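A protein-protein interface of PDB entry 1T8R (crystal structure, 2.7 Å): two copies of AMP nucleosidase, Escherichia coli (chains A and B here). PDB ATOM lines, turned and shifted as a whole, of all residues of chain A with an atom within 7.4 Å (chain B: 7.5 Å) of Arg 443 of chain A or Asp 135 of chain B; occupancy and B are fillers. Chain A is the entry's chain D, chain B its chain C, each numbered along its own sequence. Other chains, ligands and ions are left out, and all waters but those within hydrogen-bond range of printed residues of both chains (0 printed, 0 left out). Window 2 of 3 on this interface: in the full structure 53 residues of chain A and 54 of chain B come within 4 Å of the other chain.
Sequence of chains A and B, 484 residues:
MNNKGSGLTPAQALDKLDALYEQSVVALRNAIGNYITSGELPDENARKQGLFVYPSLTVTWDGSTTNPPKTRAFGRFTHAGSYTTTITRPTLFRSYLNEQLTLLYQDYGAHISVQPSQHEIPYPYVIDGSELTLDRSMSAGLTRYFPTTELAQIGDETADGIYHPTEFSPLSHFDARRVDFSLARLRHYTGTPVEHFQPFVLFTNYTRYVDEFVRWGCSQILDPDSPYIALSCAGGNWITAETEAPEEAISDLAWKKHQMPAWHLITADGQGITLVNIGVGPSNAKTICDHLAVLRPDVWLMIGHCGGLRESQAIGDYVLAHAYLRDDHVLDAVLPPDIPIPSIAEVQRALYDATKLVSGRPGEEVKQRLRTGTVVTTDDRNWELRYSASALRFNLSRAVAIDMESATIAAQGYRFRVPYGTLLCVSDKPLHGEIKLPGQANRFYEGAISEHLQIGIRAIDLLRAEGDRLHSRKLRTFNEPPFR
No position is printed for both chains. Of the 7 pairs that touch across the chains among the printed residues, none has its exchanged pair printed and touching as well.
The backbone carbonyl oxygen (O) of Ile 315 of chain A is in hydrogen-bond range of the guanidinium group (NH2) of Arg 136 of chain B (3.1 Å). The guanidinium group (NE) of Arg 443 of chain A is in hydrogen-bond range of the backbone carbonyl oxygen (O) of Thr 133 of chain B, 3.1 Å away.
OD1 of Asp 135 of chain B is in hydrogen-bond range of N of Met 138 of chain B (2.9 Å). The side-chain carboxylate (OD1) of Asp 135 of chain B lies within hydrogen-bond range of the backbone NH (N) of Ser 137 of chain B (2.8 Å). The backbone carbonyl oxygen of Asp 135 of chain B sits at hydrogen-bond distance from the side-chain hydroxyl of Ser 139 of chain B (3.4 Å).
Printed residues of chain B within 4 Å of Ile 315 of chain A: Arg 136 (3.1 Å). Arg 443 of chain A touches just these residues of chain B: Thr 133, Leu 134 and Asp 135. Of the printed residues of chain B, Phe 444 of chain A touches Leu 134 (3.6 Å), Asp 135 (3.9 Å) and Arg 136 (3.0 Å). Printed residues of chain A within 4 Å of Thr 133 of chain B: Arg 443. Printed residues of chain A within 4 Å of Leu 134 of chain B: Arg 443 (3.5 Å) and Phe 444 (3.6 Å). Printed residues of chain A within 4 Å of Arg 136 of chain B: Ile 315 and Phe 444. The nearest printed residue of chain A that does not touch Arg 136 of chain B is Arg 443 of chain A (5.0 Å).
Of the 11 printed residues of chain A, 3 touch a printed residue of chain B. Hydrophobic or aromatic side chains of chain A within 4 Å of the printed part of chain B: Phe 444. Printed residues of chain B that touch a printed residue of chain A: Thr 133, Leu 134, Asp 135 and Arg 136.
NE of Arg 443 of chain A touches O of Leu 134 of chain B, 3.5 Å away. CA of Asp 135 of chain B touches NH2 of Arg 443 of chain A (3.5 Å). Phe 444 of chain A touches Leu 134 of chain B. Phe 444 of chain A touches Asp 135 of chain B (CZ to CA, 3.9 Å). Arg 136 of chain B touches Phe 444 of chain A (NH2 to CD2, 3.0 Å).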
ATOM      1  N   ILE A 315      13.860  22.849   2.349  1.00  0.00           N
ATOM      2  CA  ILE A 315      12.770  23.318   1.529  1.00  0.00           C
ATOM      3  C   ILE A 315      12.417  24.706   2.023  1.00  0.00           C
ATOM      4  O   ILE A 315      12.268  24.917   3.218  1.00  0.00           O
ATOM      5  CB  ILE A 315      11.557  22.389   1.630  1.00  0.00           C
ATOM      6  CG1 ILE A 315      11.873  21.082   0.904  1.00  0.00           C
ATOM      7  CG2 ILE A 315      10.347  23.059   1.034  1.00  0.00           C
ATOM      8  CD1 ILE A 315      10.742  20.095   0.867  1.00  0.00           C
ATOM      9  N   LYS A 436       8.660  16.400  -4.120  1.00  0.00           N
ATOM     10  CA  LYS A 436       7.353  17.049  -3.952  1.00  0.00           C
ATOM     11  C   LYS A 436       7.023  17.725  -5.280  1.00  0.00           C
ATOM     12  O   LYS A 436       7.931  18.130  -6.009  1.00  0.00           O
ATOM     13  CB  LYS A 436       7.408  18.125  -2.861  1.00  0.00           C
ATOM     14  CG  LYS A 436       8.128  17.736  -1.567  1.00  0.00           C
ATOM     15  CD  LYS A 436       7.364  16.724  -0.713  1.00  0.00           C
ATOM     16  CE  LYS A 436       6.033  17.269  -0.214  1.00  0.00           C
ATOM     17  NZ  LYS A 436       5.005  17.342  -1.298  1.00  0.00           N
ATOM     18  N   GLN A 440       1.082  20.071  -4.837  1.00  0.00           N
ATOM     19  CA  GLN A 440       0.917  19.007  -3.853  1.00  0.00           C
ATOM     20  C   GLN A 440       1.032  19.670  -2.472  1.00  0.00           C
ATOM     21  O   GLN A 440       1.435  20.835  -2.363  1.00  0.00           O
ATOM     22  CB  GLN A 440       2.004  17.928  -4.011  1.00  0.00           C
ATOM     23  CG  GLN A 440       1.883  17.034  -5.261  1.00  0.00           C
ATOM     24  CD  GLN A 440       2.969  15.941  -5.331  1.00  0.00           C
ATOM     25  OE1 GLN A 440       3.096  15.228  -6.333  1.00  0.00           O
ATOM     26  NE2 GLN A 440       3.747  15.810  -4.261  1.00  0.00           N
ATOM     27  N   ALA A 441       0.675  18.945  -1.420  1.00  0.00           N
ATOM     28  CA  ALA A 441       0.764  19.514  -0.084  1.00  0.00           C
ATOM     29  C   ALA A 441       2.228  19.622   0.345  1.00  0.00           C
ATOM     30  O   ALA A 441       2.885  18.613   0.615  1.00  0.00           O
ATOM     31  CB  ALA A 441      -0.008  18.662   0.897  1.00  0.00           C
ATOM     32  N   ASN A 442       2.731  20.855   0.380  1.00  0.00           N
ATOM     33  CA  ASN A 442       4.107  21.150   0.778  1.00  0.00           C
ATOM     34  C   ASN A 442       4.049  22.336   1.744  1.00  0.00           C
ATOM     35  O   ASN A 442       4.083  23.503   1.345  1.00  0.00           O
ATOM     36  CB  ASN A 442       4.951  21.515  -0.445  1.00  0.00           C
ATOM     37  CG  ASN A 442       6.437  21.565  -0.140  1.00  0.00           C
ATOM     38  OD1 ASN A 442       6.858  21.648   1.018  1.00  0.00           O
ATOM     39  ND2 ASN A 442       7.244  21.524  -1.188  1.00  0.00           N
ATOM     40  N   ARG A 443       3.951  22.009   3.022  1.00  0.00           N
ATOM     41  CA  ARG A 443       3.854  22.987   4.092  1.00  0.00           C
ATOM     42  C   ARG A 443       4.911  24.087   4.066  1.00  0.00           C
ATOM     43  O   ARG A 443       4.591  25.275   4.129  1.00  0.00           O
ATOM     44  CB  ARG A 443       3.894  22.235   5.432  1.00  0.00           C
ATOM     45  CG  ARG A 443       3.775  23.052   6.703  1.00  0.00           C
ATOM     46  CD  ARG A 443       3.038  22.204   7.743  1.00  0.00           C
ATOM     47  NE  ARG A 443       3.735  22.010   9.015  1.00  0.00           N
ATOM     48  CZ  ARG A 443       4.048  22.990   9.855  1.00  0.00           C
ATOM     49  NH1 ARG A 443       3.734  24.246   9.560  1.00  0.00           N
ATOM     50  NH2 ARG A 443       4.656  22.714  11.002  1.00  0.00           N
ATOM     51  N   PHE A 444       6.173  23.709   3.939  1.00  0.00           N
ATOM     52  CA  PHE A 444       7.208  24.727   3.983  1.00  0.00           C
ATOM     53  C   PHE A 444       7.537  25.502   2.719  1.00  0.00           C
ATOM     54  O   PHE A 444       8.182  26.550   2.792  1.00  0.00           O
ATOM     55  CB  PHE A 444       8.461  24.137   4.627  1.00  0.00           C
ATOM     56  CG  PHE A 444       8.224  23.653   6.024  1.00  0.00           C
ATOM     57  CD1 PHE A 444       7.949  22.312   6.269  1.00  0.00           C
ATOM     58  CD2 PHE A 444       8.206  24.557   7.087  1.00  0.00           C
ATOM     59  CE1 PHE A 444       7.659  21.873   7.549  1.00  0.00           C
ATOM     60  CE2 PHE A 444       7.917  24.135   8.379  1.00  0.00           C
ATOM     61  CZ  PHE A 444       7.640  22.785   8.615  1.00  0.00           C
ATOM     62  N   TYR A 445       7.102  25.013   1.567  1.00  0.00           N
ATOM     63  CA  TYR A 445       7.336  25.771   0.353  1.00  0.00           C
ATOM     64  C   TYR A 445       6.164  26.741   0.165  1.00  0.00           C
ATOM     65  O   TYR A 445       6.370  27.910  -0.146  1.00  0.00           O
ATOM     66  CB  TYR A 445       7.474  24.861  -0.868  1.00  0.00           C
ATOM     67  CG  TYR A 445       7.422  25.629  -2.165  1.00  0.00           C
ATOM     68  CD1 TYR A 445       8.273  26.712  -2.396  1.00  0.00           C
ATOM     69  CD2 TYR A 445       6.474  25.316  -3.137  1.00  0.00           C
ATOM     70  CE1 TYR A 445       8.172  27.477  -3.570  1.00  0.00           C
ATOM     71  CE2 TYR A 445       6.363  26.069  -4.312  1.00  0.00           C
ATOM     72  CZ  TYR A 445       7.214  27.146  -4.518  1.00  0.00           C
ATOM     73  OH  TYR A 445       7.084  27.873  -5.673  1.00  0.00           O
ATOM     74  N   GLU A 446       4.938  26.257   0.359  1.00  0.00           N
ATOM     75  CA  GLU A 446       3.746  27.107   0.227  1.00  0.00           C
ATOM     76  C   GLU A 446       3.870  28.250   1.221  1.00  0.00           C
ATOM     77  O   GLU A 446       3.452  29.369   0.955  1.00  0.00           O
ATOM     78  CB  GLU A 446       2.467  26.328   0.543  1.00  0.00           C
ATOM     79  CG  GLU A 446       2.121  25.212  -0.432  1.00  0.00           C
ATOM     80  CD  GLU A 446       1.588  25.720  -1.780  1.00  0.00           C
ATOM     81  OE1 GLU A 446       0.749  26.661  -1.787  1.00  0.00           O
ATOM     82  OE2 GLU A 446       1.993  25.156  -2.833  1.00  0.00           O
ATOM     83  N   GLY A 447       4.461  27.966   2.372  1.00  0.00           N
ATOM     84  CA  GLY A 447       4.617  29.014   3.354  1.00  0.00           C
ATOM     85  C   GLY A 447       5.664  30.038   2.974  1.00  0.00           C
ATOM     86  O   GLY A 447       5.740  31.100   3.586  1.00  0.00           O
ATOM     87  N   ALA A 448       6.473  29.746   1.963  1.00  0.00           N
ATOM     88  CA  ALA A 448       7.520  30.679   1.573  1.00  0.00           C
ATOM     89  C   ALA A 448       7.129  31.539   0.388  1.00  0.00           C
ATOM     90  O   ALA A 448       7.717  32.593   0.147  1.00  0.00           O
ATOM     91  CB  ALA A 448       8.801  29.915   1.257  1.00  0.00           C
ATOM     92  N   LEU B 132       1.720  14.166   3.571  1.00  0.00           N
ATOM     93  CA  LEU B 132       1.882  14.555   4.969  1.00  0.00           C
ATOM     94  C   LEU B 132       2.422  15.970   5.135  1.00  0.00           C
ATOM     95  O   LEU B 132       3.179  16.450   4.297  1.00  0.00           O
ATOM     96  CB  LEU B 132       2.794  13.569   5.697  1.00  0.00           C
ATOM     97  CG  LEU B 132       2.148  12.234   6.070  1.00  0.00           C
ATOM     98  CD1 LEU B 132       3.162  11.383   6.810  1.00  0.00           C
ATOM     99  CD2 LEU B 132       0.916  12.467   6.937  1.00  0.00           C
ATOM    100  N   THR B 133       2.029  16.631   6.223  1.00  0.00           N
ATOM    101  CA  THR B 133       2.461  17.999   6.489  1.00  0.00           C
ATOM    102  C   THR B 133       2.890  18.254   7.941  1.00  0.00           C
ATOM    103  O   THR B 133       2.443  19.199   8.589  1.00  0.00           O
ATOM    104  CB  THR B 133       1.356  19.023   6.079  1.00  0.00           C
ATOM    105  OG1 THR B 133       0.055  18.434   6.236  1.00  0.00           O
ATOM    106  CG2 THR B 133       1.546  19.464   4.631  1.00  0.00           C
ATOM    107  N   LEU B 134       3.769  17.390   8.432  1.00  0.00           N
ATOM    108  CA  LEU B 134       4.341  17.446   9.775  1.00  0.00           C
ATOM    109  C   LEU B 134       5.362  18.580   9.833  1.00  0.00           C
ATOM    110  O   LEU B 134       5.747  19.113   8.801  1.00  0.00           O
ATOM    111  CB  LEU B 134       5.049  16.123  10.067  1.00  0.00           C
ATOM    112  CG  LEU B 134       4.248  14.815  10.129  1.00  0.00           C
ATOM    113  CD1 LEU B 134       3.393  14.621   8.889  1.00  0.00           C
ATOM    114  CD2 LEU B 134       5.222  13.665  10.279  1.00  0.00           C
ATOM    115  N   ASP B 135       5.805  18.943  11.032  1.00  0.00           N
ATOM    116  CA  ASP B 135       6.795  20.006  11.177  1.00  0.00           C
ATOM    117  C   ASP B 135       8.120  19.502  10.623  1.00  0.00           C
ATOM    118  O   ASP B 135       8.251  18.325  10.308  1.00  0.00           O
ATOM    119  CB  ASP B 135       6.955  20.409  12.649  1.00  0.00           C
ATOM    120  CG  ASP B 135       7.509  19.286  13.516  1.00  0.00           C
ATOM    121  OD1 ASP B 135       8.685  18.912  13.330  1.00  0.00           O
ATOM    122  OD2 ASP B 135       6.769  18.777  14.386  1.00  0.00           O
ATOM    123  N   ARG B 136       9.100  20.391  10.512  1.00  0.00           N
ATOM    124  CA  ARG B 136      10.404  20.023   9.969  1.00  0.00           C
ATOM    125  C   ARG B 136      11.060  18.856  10.684  1.00  0.00           C
ATOM    126  O   ARG B 136      11.473  17.891  10.048  1.00  0.00           O
ATOM    127  CB  ARG B 136      11.345  21.231   9.973  1.00  0.00           C
ATOM    128  CG  ARG B 136      10.932  22.306   8.986  1.00  0.00           C
ATOM    129  CD  ARG B 136      11.907  23.456   8.955  1.00  0.00           C
ATOM    130  NE  ARG B 136      11.457  24.511   8.052  1.00  0.00           N
ATOM    131  CZ  ARG B 136      11.320  24.370   6.737  1.00  0.00           C
ATOM    132  NH1 ARG B 136      11.596  23.209   6.151  1.00  0.00           N
ATOM    133  NH2 ARG B 136      10.904  25.397   6.008  1.00  0.00           N
ATOM    134  N   SER B 137      11.155  18.939  12.003  1.00  0.00           N
ATOM    135  CA  SER B 137      11.772  17.873  12.784  1.00  0.00           C
ATOM    136  C   SER B 137      11.156  16.502  12.488  1.00  0.00           C
ATOM    137  O   SER B 137      11.866  15.499  12.397  1.00  0.00           O
ATOM    138  CB  SER B 137      11.651  18.187  14.273  1.00  0.00           C
ATOM    139  OG  SER B 137      12.320  17.212  15.048  1.00  0.00           O
ATOM    140  N   MET B 138       9.835  16.470  12.337  1.00  0.00           N
ATOM    141  CA  MET B 138       9.104  15.239  12.048  1.00  0.00           C
ATOM    142  C   MET B 138       9.389  14.696  10.649  1.00  0.00           C
ATOM    143  O   MET B 138       9.613  13.500  10.472  1.00  0.00           O
ATOM    144  CB  MET B 138       7.596  15.483  12.194  1.00  0.00           C
ATOM    145  CG  MET B 138       7.042  15.435  13.627  1.00  0.00           C
ATOM    146  SD  MET B 138       6.493  13.641  14.220  1.00  0.00           S
ATOM    147  CE  MET B 138       4.655  13.653  13.657  1.00  0.00           C
ATOM    148  N   SER B 139       9.364  15.577   9.655  1.00  0.00           N
ATOM    149  CA  SER B 139       9.607  15.179   8.274  1.00  0.00           C
ATOM    150  C   SER B 139      11.015  14.660   8.124  1.00  0.00           C
ATOM    151  O   SER B 139      11.251  13.668   7.446  1.00  0.00           O
ATOM    152  CB  SER B 139       9.399  16.359   7.321  1.00  0.00           C
ATOM    153  OG  SER B 139       8.046  16.779   7.300  1.00  0.00           O
ATOM    154  N   ALA B 140      11.954  15.348   8.757  1.00  0.00           N
ATOM    155  CA  ALA B 140      13.357  14.957   8.704  1.00  0.00           C
ATOM    156  C   ALA B 140      13.511  13.541   9.244  1.00  0.00           C
ATOM    157  O   ALA B 140      14.308  12.751   8.736  1.00  0.00           O
ATOM    158  CB  ALA B 140      14.203  15.924   9.520  1.00  0.00           C
ATOM    159  N   GLY B 141      12.739  13.229  10.277  1.00  0.00           N
ATOM    160  CA  GLY B 141      12.796  11.911  10.866  1.00  0.00           C
ATOM    161  C   GLY B 141      12.224  10.849   9.959  1.00  0.00           C
ATOM    162  O   GLY B 141      12.761   9.750   9.884  1.00  0.00           O
